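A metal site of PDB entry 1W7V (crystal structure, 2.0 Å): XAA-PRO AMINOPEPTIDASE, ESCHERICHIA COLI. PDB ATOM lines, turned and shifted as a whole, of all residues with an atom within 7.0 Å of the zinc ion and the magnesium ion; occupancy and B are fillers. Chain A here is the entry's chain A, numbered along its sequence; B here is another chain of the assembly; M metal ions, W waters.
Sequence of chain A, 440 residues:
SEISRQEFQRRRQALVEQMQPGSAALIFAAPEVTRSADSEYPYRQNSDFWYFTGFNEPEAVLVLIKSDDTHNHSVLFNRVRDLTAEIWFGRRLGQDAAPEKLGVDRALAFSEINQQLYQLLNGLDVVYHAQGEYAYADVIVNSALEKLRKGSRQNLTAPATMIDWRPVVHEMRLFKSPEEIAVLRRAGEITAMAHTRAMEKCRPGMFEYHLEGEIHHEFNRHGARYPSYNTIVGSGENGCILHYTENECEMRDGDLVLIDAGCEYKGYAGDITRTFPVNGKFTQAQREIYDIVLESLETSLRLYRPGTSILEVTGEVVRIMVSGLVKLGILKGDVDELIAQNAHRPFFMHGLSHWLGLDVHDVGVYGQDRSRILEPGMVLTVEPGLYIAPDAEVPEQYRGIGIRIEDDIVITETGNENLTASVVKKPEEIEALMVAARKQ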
ATOM      1  N   TYR A 229     -29.583  -9.273  22.279  1.00  0.00           N
ATOM      2  CA  TYR A 229     -29.496  -9.097  23.726  1.00  0.00           C
ATOM      3  C   TYR A 229     -30.036  -7.696  24.056  1.00  0.00           C
ATOM      4  O   TYR A 229     -30.203  -6.864  23.173  1.00  0.00           O
ATOM      5  CB  TYR A 229     -28.045  -9.222  24.237  1.00  0.00           C
ATOM      6  CG  TYR A 229     -27.075  -8.336  23.507  1.00  0.00           C
ATOM      7  CD1 TYR A 229     -26.524  -8.738  22.295  1.00  0.00           C
ATOM      8  CD2 TYR A 229     -26.740  -7.077  23.983  1.00  0.00           C
ATOM      9  CE1 TYR A 229     -25.634  -7.925  21.603  1.00  0.00           C
ATOM     10  CE2 TYR A 229     -25.845  -6.251  23.286  1.00  0.00           C
ATOM     11  CZ  TYR A 229     -25.292  -6.690  22.110  1.00  0.00           C
ATOM     12  OH  TYR A 229     -24.419  -5.894  21.394  1.00  0.00           O
ATOM     13  N   ILE A 232     -27.617  -1.768  25.587  1.00  0.00           N
ATOM     14  CA  ILE A 232     -26.977  -0.954  26.627  1.00  0.00           C
ATOM     15  C   ILE A 232     -26.647   0.424  26.069  1.00  0.00           C
ATOM     16  O   ILE A 232     -25.980   0.535  25.060  1.00  0.00           O
ATOM     17  CB  ILE A 232     -25.670  -1.645  27.056  1.00  0.00           C
ATOM     18  CG1 ILE A 232     -25.969  -2.976  27.762  1.00  0.00           C
ATOM     19  CG2 ILE A 232     -24.767  -0.708  27.914  1.00  0.00           C
ATOM     20  CD1 ILE A 232     -24.812  -3.966  27.752  1.00  0.00           C
ATOM     21  N   ILE A 259     -22.450   2.519  23.855  1.00  0.00           N
ATOM     22  CA  ILE A 259     -23.575   1.766  23.271  1.00  0.00           C
ATOM     23  C   ILE A 259     -23.131   0.378  22.882  1.00  0.00           C
ATOM     24  O   ILE A 259     -22.286   0.223  22.023  1.00  0.00           O
ATOM     25  CB  ILE A 259     -24.171   2.459  22.061  1.00  0.00           C
ATOM     26  CG1 ILE A 259     -24.608   3.884  22.426  1.00  0.00           C
ATOM     27  CG2 ILE A 259     -25.369   1.662  21.536  1.00  0.00           C
ATOM     28  CD1 ILE A 259     -25.374   4.606  21.343  1.00  0.00           C
ATOM     29  N   ASP A 260     -23.713  -0.621  23.539  1.00  0.00           N
ATOM     30  CA  ASP A 260     -23.492  -2.019  23.191  1.00  0.00           C
ATOM     31  C   ASP A 260     -24.817  -2.574  22.693  1.00  0.00           C
ATOM     32  O   ASP A 260     -25.770  -2.695  23.459  1.00  0.00           O
ATOM     33  CB  ASP A 260     -22.965  -2.800  24.411  1.00  0.00           C
ATOM     34  CG  ASP A 260     -22.362  -4.158  24.049  1.00  0.00           C
ATOM     35  OD1 ASP A 260     -22.611  -4.684  22.931  1.00  0.00           O
ATOM     36  OD2 ASP A 260     -21.606  -4.725  24.869  1.00  0.00           O
ATOM     37  N   ALA A 261     -24.890  -2.881  21.399  1.00  0.00           N
ATOM     38  CA  ALA A 261     -26.136  -3.306  20.792  1.00  0.00           C
ATOM     39  C   ALA A 261     -25.846  -4.222  19.619  1.00  0.00           C
ATOM     40  O   ALA A 261     -24.837  -4.054  18.917  1.00  0.00           O
ATOM     41  CB  ALA A 261     -26.941  -2.109  20.305  1.00  0.00           C
ATOM     42  N   GLY A 262     -26.747  -5.181  19.392  1.00  0.00           N
ATOM     43  CA  GLY A 262     -26.606  -6.121  18.310  1.00  0.00           C
ATOM     44  C   GLY A 262     -27.938  -6.680  17.863  1.00  0.00           C
ATOM     45  O   GLY A 262     -28.841  -6.881  18.671  1.00  0.00           O
ATOM     46  N   GLY A 270     -25.391 -10.174  15.970  1.00  0.00           N
ATOM     47  CA  GLY A 270     -24.358  -9.123  15.930  1.00  0.00           C
ATOM     48  C   GLY A 270     -24.068  -8.690  17.367  1.00  0.00           C
ATOM     49  O   GLY A 270     -24.892  -8.890  18.275  1.00  0.00           O
ATOM     50  N   ASP A 271     -22.909  -8.085  17.591  1.00  0.00           N
ATOM     51  CA  ASP A 271     -22.528  -7.638  18.928  1.00  0.00           C
ATOM     52  C   ASP A 271     -21.428  -6.570  18.808  1.00  0.00           C
ATOM     53  O   ASP A 271     -20.249  -6.878  18.714  1.00  0.00           O
ATOM     54  CB  ASP A 271     -22.076  -8.852  19.741  1.00  0.00           C
ATOM     55  CG  ASP A 271     -21.690  -8.527  21.175  1.00  0.00           C
ATOM     56  OD1 ASP A 271     -21.824  -7.388  21.700  1.00  0.00           O
ATOM     57  OD2 ASP A 271     -21.204  -9.471  21.806  1.00  0.00           O
ATOM     58  N   ILE A 272     -21.857  -5.310  18.780  1.00  0.00           N
ATOM     59  CA  ILE A 272     -20.945  -4.174  18.600  1.00  0.00           C
ATOM     60  C   ILE A 272     -21.075  -3.215  19.772  1.00  0.00           C
ATOM     61  O   ILE A 272     -22.181  -2.972  20.278  1.00  0.00           O
ATOM     62  CB  ILE A 272     -21.213  -3.393  17.283  1.00  0.00           C
ATOM     63  CG1 ILE A 272     -20.947  -4.273  16.066  1.00  0.00           C
ATOM     64  CG2 ILE A 272     -20.367  -2.105  17.200  1.00  0.00           C
ATOM     65  CD1 ILE A 272     -21.252  -3.570  14.734  1.00  0.00           C
ATOM     66  N   THR A 273     -19.928  -2.694  20.204  1.00  0.00           N
ATOM     67  CA  THR A 273     -19.898  -1.596  21.140  1.00  0.00           C
ATOM     68  C   THR A 273     -19.108  -0.431  20.542  1.00  0.00           C
ATOM     69  O   THR A 273     -18.023  -0.609  19.989  1.00  0.00           O
ATOM     70  CB  THR A 273     -19.264  -1.946  22.498  1.00  0.00           C
ATOM     71  OG1 THR A 273     -19.903  -3.112  23.048  1.00  0.00           O
ATOM     72  CG2 THR A 273     -19.440  -0.788  23.489  1.00  0.00           C
ATOM     73  N   SER A 353     -12.669 -11.496  24.686  1.00  0.00           N
ATOM     74  CA  SER A 353     -13.338 -12.133  23.560  1.00  0.00           C
ATOM     75  C   SER A 353     -14.261 -13.248  24.019  1.00  0.00           C
ATOM     76  O   SER A 353     -13.919 -13.991  24.934  1.00  0.00           O
ATOM     77  CB  SER A 353     -12.279 -12.765  22.624  1.00  0.00           C
ATOM     78  OG  SER A 353     -11.496 -11.793  21.951  1.00  0.00           O
ATOM     79  N   HIS A 354     -15.405 -13.383  23.374  1.00  0.00           N
ATOM     80  CA  HIS A 354     -16.246 -14.564  23.516  1.00  0.00           C
ATOM     81  C   HIS A 354     -16.668 -15.035  22.129  1.00  0.00           C
ATOM     82  O   HIS A 354     -16.654 -14.269  21.166  1.00  0.00           O
ATOM     83  CB  HIS A 354     -17.480 -14.281  24.394  1.00  0.00           C
ATOM     84  CG  HIS A 354     -18.358 -13.181  23.884  1.00  0.00           C
ATOM     85  ND1 HIS A 354     -19.284 -13.367  22.878  1.00  0.00           N
ATOM     86  CD2 HIS A 354     -18.434 -11.869  24.235  1.00  0.00           C
ATOM     87  CE1 HIS A 354     -19.885 -12.207  22.626  1.00  0.00           C
ATOM     88  NE2 HIS A 354     -19.394 -11.299  23.450  1.00  0.00           N
ATOM     89  N   TRP A 355     -17.025 -16.314  22.032  1.00  0.00           N
ATOM     90  CA  TRP A 355     -17.581 -16.865  20.806  1.00  0.00           C
ATOM     91  C   TRP A 355     -18.884 -16.162  20.464  1.00  0.00           C
ATOM     92  O   TRP A 355     -19.598 -15.672  21.353  1.00  0.00           O
ATOM     93  CB  TRP A 355     -17.899 -18.359  20.931  1.00  0.00           C
ATOM     94  CG  TRP A 355     -16.817 -19.283  21.432  1.00  0.00           C
ATOM     95  CD1 TRP A 355     -16.950 -20.222  22.401  1.00  0.00           C
ATOM     96  CD2 TRP A 355     -15.446 -19.372  20.977  1.00  0.00           C
ATOM     97  NE1 TRP A 355     -15.774 -20.892  22.591  1.00  0.00           N
ATOM     98  CE2 TRP A 355     -14.833 -20.389  21.742  1.00  0.00           C
ATOM     99  CE3 TRP A 355     -14.682 -18.692  20.024  1.00  0.00           C
ATOM    100  CZ2 TRP A 355     -13.483 -20.747  21.558  1.00  0.00           C
ATOM    101  CZ3 TRP A 355     -13.360 -19.041  19.852  1.00  0.00           C
ATOM    102  CH2 TRP A 355     -12.775 -20.061  20.621  1.00  0.00           C
ATOM    103  N   LEU A 356     -19.216 -16.150  19.183  1.00  0.00           N
ATOM    104  CA  LEU A 356     -20.414 -15.487  18.695  1.00  0.00           C
ATOM    105  C   LEU A 356     -21.097 -16.380  17.653  1.00  0.00           C
ATOM    106  O   LEU A 356     -20.427 -17.025  16.846  1.00  0.00           O
ATOM    107  CB  LEU A 356     -20.001 -14.157  18.080  1.00  0.00           C
ATOM    108  CG  LEU A 356     -21.083 -13.224  17.534  1.00  0.00           C
ATOM    109  CD1 LEU A 356     -21.865 -12.563  18.666  1.00  0.00           C
ATOM    110  CD2 LEU A 356     -20.431 -12.181  16.649  1.00  0.00           C
ATOM    111  N   VAL A 360     -25.379 -14.895  21.513  1.00  0.00           N
ATOM    112  CA  VAL A 360     -24.397 -13.825  21.576  1.00  0.00           C
ATOM    113  C   VAL A 360     -23.164 -14.266  22.351  1.00  0.00           C
ATOM    114  O   VAL A 360     -22.053 -13.996  21.928  1.00  0.00           O
ATOM    115  CB  VAL A 360     -24.992 -12.495  22.122  1.00  0.00           C
ATOM    116  CG1 VAL A 360     -25.494 -12.634  23.513  1.00  0.00           C
ATOM    117  CG2 VAL A 360     -23.927 -11.381  22.046  1.00  0.00           C
ATOM    118  N   HIS A 361     -23.356 -14.953  23.482  1.00  0.00           N
ATOM    119  CA  HIS A 361     -22.263 -15.661  24.154  1.00  0.00           C
ATOM    120  C   HIS A 361     -22.396 -17.102  23.708  1.00  0.00           C
ATOM    121  O   HIS A 361     -23.130 -17.884  24.312  1.00  0.00           O
ATOM    122  CB  HIS A 361     -22.361 -15.540  25.675  1.00  0.00           C
ATOM    123  CG  HIS A 361     -22.172 -14.145  26.176  1.00  0.00           C
ATOM    124  ND1 HIS A 361     -22.678 -13.708  27.378  1.00  0.00           N
ATOM    125  CD2 HIS A 361     -21.587 -13.063  25.597  1.00  0.00           C
ATOM    126  CE1 HIS A 361     -22.377 -12.432  27.538  1.00  0.00           C
ATOM    127  NE2 HIS A 361     -21.725 -12.017  26.477  1.00  0.00           N
ATOM    128  N   THR A 381     -15.820 -12.154  19.382  1.00  0.00           N
ATOM    129  CA  THR A 381     -15.758 -10.721  19.577  1.00  0.00           C
ATOM    130  C   THR A 381     -14.376 -10.323  20.067  1.00  0.00           C
ATOM    131  O   THR A 381     -13.589 -11.149  20.530  1.00  0.00           O
ATOM    132  CB  THR A 381     -16.771 -10.238  20.631  1.00  0.00           C
ATOM    133  OG1 THR A 381     -16.436 -10.802  21.912  1.00  0.00           O
ATOM    134  CG2 THR A 381     -18.194 -10.655  20.201  1.00  0.00           C
ATOM    135  N   VAL A 382     -14.079  -9.033  19.914  1.00  0.00           N
ATOM    136  CA  VAL A 382     -12.886  -8.434  20.463  1.00  0.00           C
ATOM    137  C   VAL A 382     -13.365  -7.160  21.133  1.00  0.00           C
ATOM    138  O   VAL A 382     -13.846  -6.259  20.453  1.00  0.00           O
ATOM    139  CB  VAL A 382     -11.874  -8.101  19.359  1.00  0.00           C
ATOM    140  CG1 VAL A 382     -10.561  -7.635  19.958  1.00  0.00           C
ATOM    141  CG2 VAL A 382     -11.670  -9.307  18.428  1.00  0.00           C
ATOM    142  N   GLU A 383     -13.279  -7.092  22.454  1.00  0.00           N
ATOM    143  CA  GLU A 383     -13.908  -6.004  23.191  1.00  0.00           C
ATOM    144  C   GLU A 383     -13.122  -5.506  24.388  1.00  0.00           C
ATOM    145  O   GLU A 383     -13.557  -5.653  25.537  1.00  0.00           O
ATOM    146  CB  GLU A 383     -15.318  -6.370  23.617  1.00  0.00           C
ATOM    147  CG  GLU A 383     -15.483  -7.625  24.405  1.00  0.00           C
ATOM    148  CD  GLU A 383     -16.960  -7.978  24.532  1.00  0.00           C
ATOM    149  OE1 GLU A 383     -17.794  -7.066  24.836  1.00  0.00           O
ATOM    150  OE2 GLU A 383     -17.298  -9.136  24.293  1.00  0.00           O
ATOM    151  N   ARG A 404     -15.683   1.199  26.003  1.00  0.00           N
ATOM    152  CA  ARG A 404     -15.491  -0.098  25.379  1.00  0.00           C
ATOM    153  C   ARG A 404     -15.669   0.059  23.868  1.00  0.00           C
ATOM    154  O   ARG A 404     -16.481   0.858  23.415  1.00  0.00           O
ATOM    155  CB  ARG A 404     -16.468  -1.138  25.962  1.00  0.00           C
ATOM    156  CG  ARG A 404     -16.377  -2.518  25.320  1.00  0.00           C
ATOM    157  CD  ARG A 404     -17.074  -3.617  26.105  1.00  0.00           C
ATOM    158  NE  ARG A 404     -18.535  -3.521  26.145  1.00  0.00           N
ATOM    159  CZ  ARG A 404     -19.272  -3.100  27.179  1.00  0.00           C
ATOM    160  NH1 ARG A 404     -18.714  -2.700  28.322  1.00  0.00           N
ATOM    161  NH2 ARG A 404     -20.592  -3.083  27.098  1.00  0.00           N
ATOM    162  N   GLU A 406     -15.907  -2.670  20.624  1.00  0.00           N
ATOM    163  CA  GLU A 406     -16.084  -4.085  20.339  1.00  0.00           C
ATOM    164  C   GLU A 406     -16.406  -4.304  18.872  1.00  0.00           C
ATOM    165  O   GLU A 406     -17.333  -3.683  18.340  1.00  0.00           O
ATOM    166  CB  GLU A 406     -17.207  -4.640  21.224  1.00  0.00           C
ATOM    167  CG  GLU A 406     -17.741  -5.990  20.799  1.00  0.00           C
ATOM    168  CD  GLU A 406     -18.712  -6.593  21.808  1.00  0.00           C
ATOM    169  OE1 GLU A 406     -19.515  -5.837  22.422  1.00  0.00           O
ATOM    170  OE2 GLU A 406     -18.661  -7.825  21.981  1.00  0.00           O
ATOM    171  N   ASP A 407     -15.623  -5.176  18.246  1.00  0.00           N
ATOM    172  CA  ASP A 407     -15.866  -5.674  16.889  1.00  0.00           C
ATOM    173  C   ASP A 407     -16.079  -7.207  16.869  1.00  0.00           C
ATOM    174  O   ASP A 407     -15.708  -7.903  17.815  1.00  0.00           O
ATOM    175  CB  ASP A 407     -14.685  -5.326  15.968  1.00  0.00           C
ATOM    176  CG  ASP A 407     -14.772  -3.897  15.388  1.00  0.00           C
ATOM    177  OD1 ASP A 407     -15.883  -3.320  15.292  1.00  0.00           O
ATOM    178  OD2 ASP A 407     -13.713  -3.365  14.978  1.00  0.00           O
ATOM    179  N   ASP A 408     -16.677  -7.707  15.784  1.00  0.00           N
ATOM    180  CA  ASP A 408     -16.911  -9.138  15.590  1.00  0.00           C
ATOM    181  C   ASP A 408     -16.033  -9.627  14.445  1.00  0.00           C
ATOM    182  O   ASP A 408     -16.033  -9.013  13.376  1.00  0.00           O
ATOM    183  CB  ASP A 408     -18.388  -9.391  15.238  1.00  0.00           C
ATOM    184  CG  ASP A 408     -19.339  -8.807  16.242  1.00  0.00           C
ATOM    185  OD1 ASP A 408     -18.962  -8.664  17.441  1.00  0.00           O
ATOM    186  OD2 ASP A 408     -20.476  -8.475  15.852  1.00  0.00           O
ATOM    187  N   PRO B   2     -20.479  -7.993  27.658  1.00  0.00           N
ATOM    188  CA  PRO B   2     -19.190  -8.649  27.885  1.00  0.00           C
ATOM    189  C   PRO B   2     -19.302  -9.968  28.650  1.00  0.00           C
ATOM    190  O   PRO B   2     -20.262 -10.177  29.412  1.00  0.00           O
ATOM    191  CB  PRO B   2     -18.403  -7.622  28.699  1.00  0.00           C
ATOM    192  CG  PRO B   2     -18.981  -6.329  28.302  1.00  0.00           C
ATOM    193  CD  PRO B   2     -20.437  -6.580  28.050  1.00  0.00           C
ATOM    194  N   LEU B   3     -18.314 -10.838  28.448  1.00  0.00           N
ATOM    195  CA  LEU B   3     -18.185 -12.116  29.166  1.00  0.00           C
ATOM    196  C   LEU B   3     -16.768 -12.173  29.739  1.00  0.00           C
ATOM    197  O   LEU B   3     -16.517 -12.292  30.939  1.00  0.00           O
ATOM    198  CB  LEU B   3     -18.427 -13.295  28.200  1.00  0.00           C
ATOM    199  CG  LEU B   3     -18.462 -14.707  28.795  1.00  0.00           C
ATOM    200  CD1 LEU B   3     -19.861 -15.056  29.258  1.00  0.00           C
ATOM    201  CD2 LEU B   3     -17.988 -15.751  27.803  1.00  0.00           C
ATOM    202  OXT LEU B   3     -15.814 -12.080  28.963  1.00  0.00           O
HETATM  203 ZN    ZN M   1     -19.687  -9.116  23.336  1.00  0.00          ZN
HETATM  204 MG    MG M   2     -21.334  -6.410  23.345  1.00  0.00          MG
HETATM  205  O   HOH W   1     -23.018  -7.327  24.380  1.00  0.00           O
HETATM  206  O   HOH W   2     -20.323  -7.633  24.689  1.00  0.00           O
HETATM  207  O   HOH W   3     -21.719  -9.274  25.834  1.00  0.00           O
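CG2 of Thr 381 touches the zinc ion, 3.8 Å away. Within 4 Å of the zinc ion: Asp 271, His 354, Thr 381, Glu 383 and Glu 406. The nearest printed residue that does not touch the zinc ion is Pro 2 of chain B (4.5 Å).
The magnesium ion is bound by OD1 of Asp 271, water W2, OE1 of Glu 406, water W1, OD1 of Asp 260 and OD2 of Asp 260. The magnesium ion has six donor atoms within binding distance.
The side-chain carboxylate (OE2) of Glu 383 sits close to the side-chain hydroxyl (OG1) of Thr 381, at 3.0 Å. The side-chain hydroxyl (OG) of Ser 353 lies within hydrogen-bond range of the backbone carbonyl oxygen (O) of Thr 381 (2.6 Å). OG1 of Thr 273 lies within hydrogen-bond range of NE of Arg 404 (3.4 Å). N of Glu 406 sits at hydrogen-bond distance from O of Thr 273 (3.0 Å). OH of Tyr 229 lies close to N of Ala 261 (3.0 Å). The side-chain carboxylate (OE1) of Glu 383 is in salt-bridge range of the guanidinium group (NE) of Arg 404 (3.9 Å). OD2 of Asp 260 lies close to OG1 of Thr 273, at 3.0 Å. OH of Tyr 229 lies close to OD1 of Asp 271, at 3.0 Å.
The zinc ion is bound by water W2, the side-chain carboxylate of Glu 406, the side-chain carboxylate of Asp 271, a ring nitrogen (NE2) of His 354 and the side-chain carboxylate of Glu 383.
Merely in contact with the magnesium ion: Tyr 229 and Thr 273. Of the 25 residues printed, 6 come within 4 Å of the magnesium ion.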
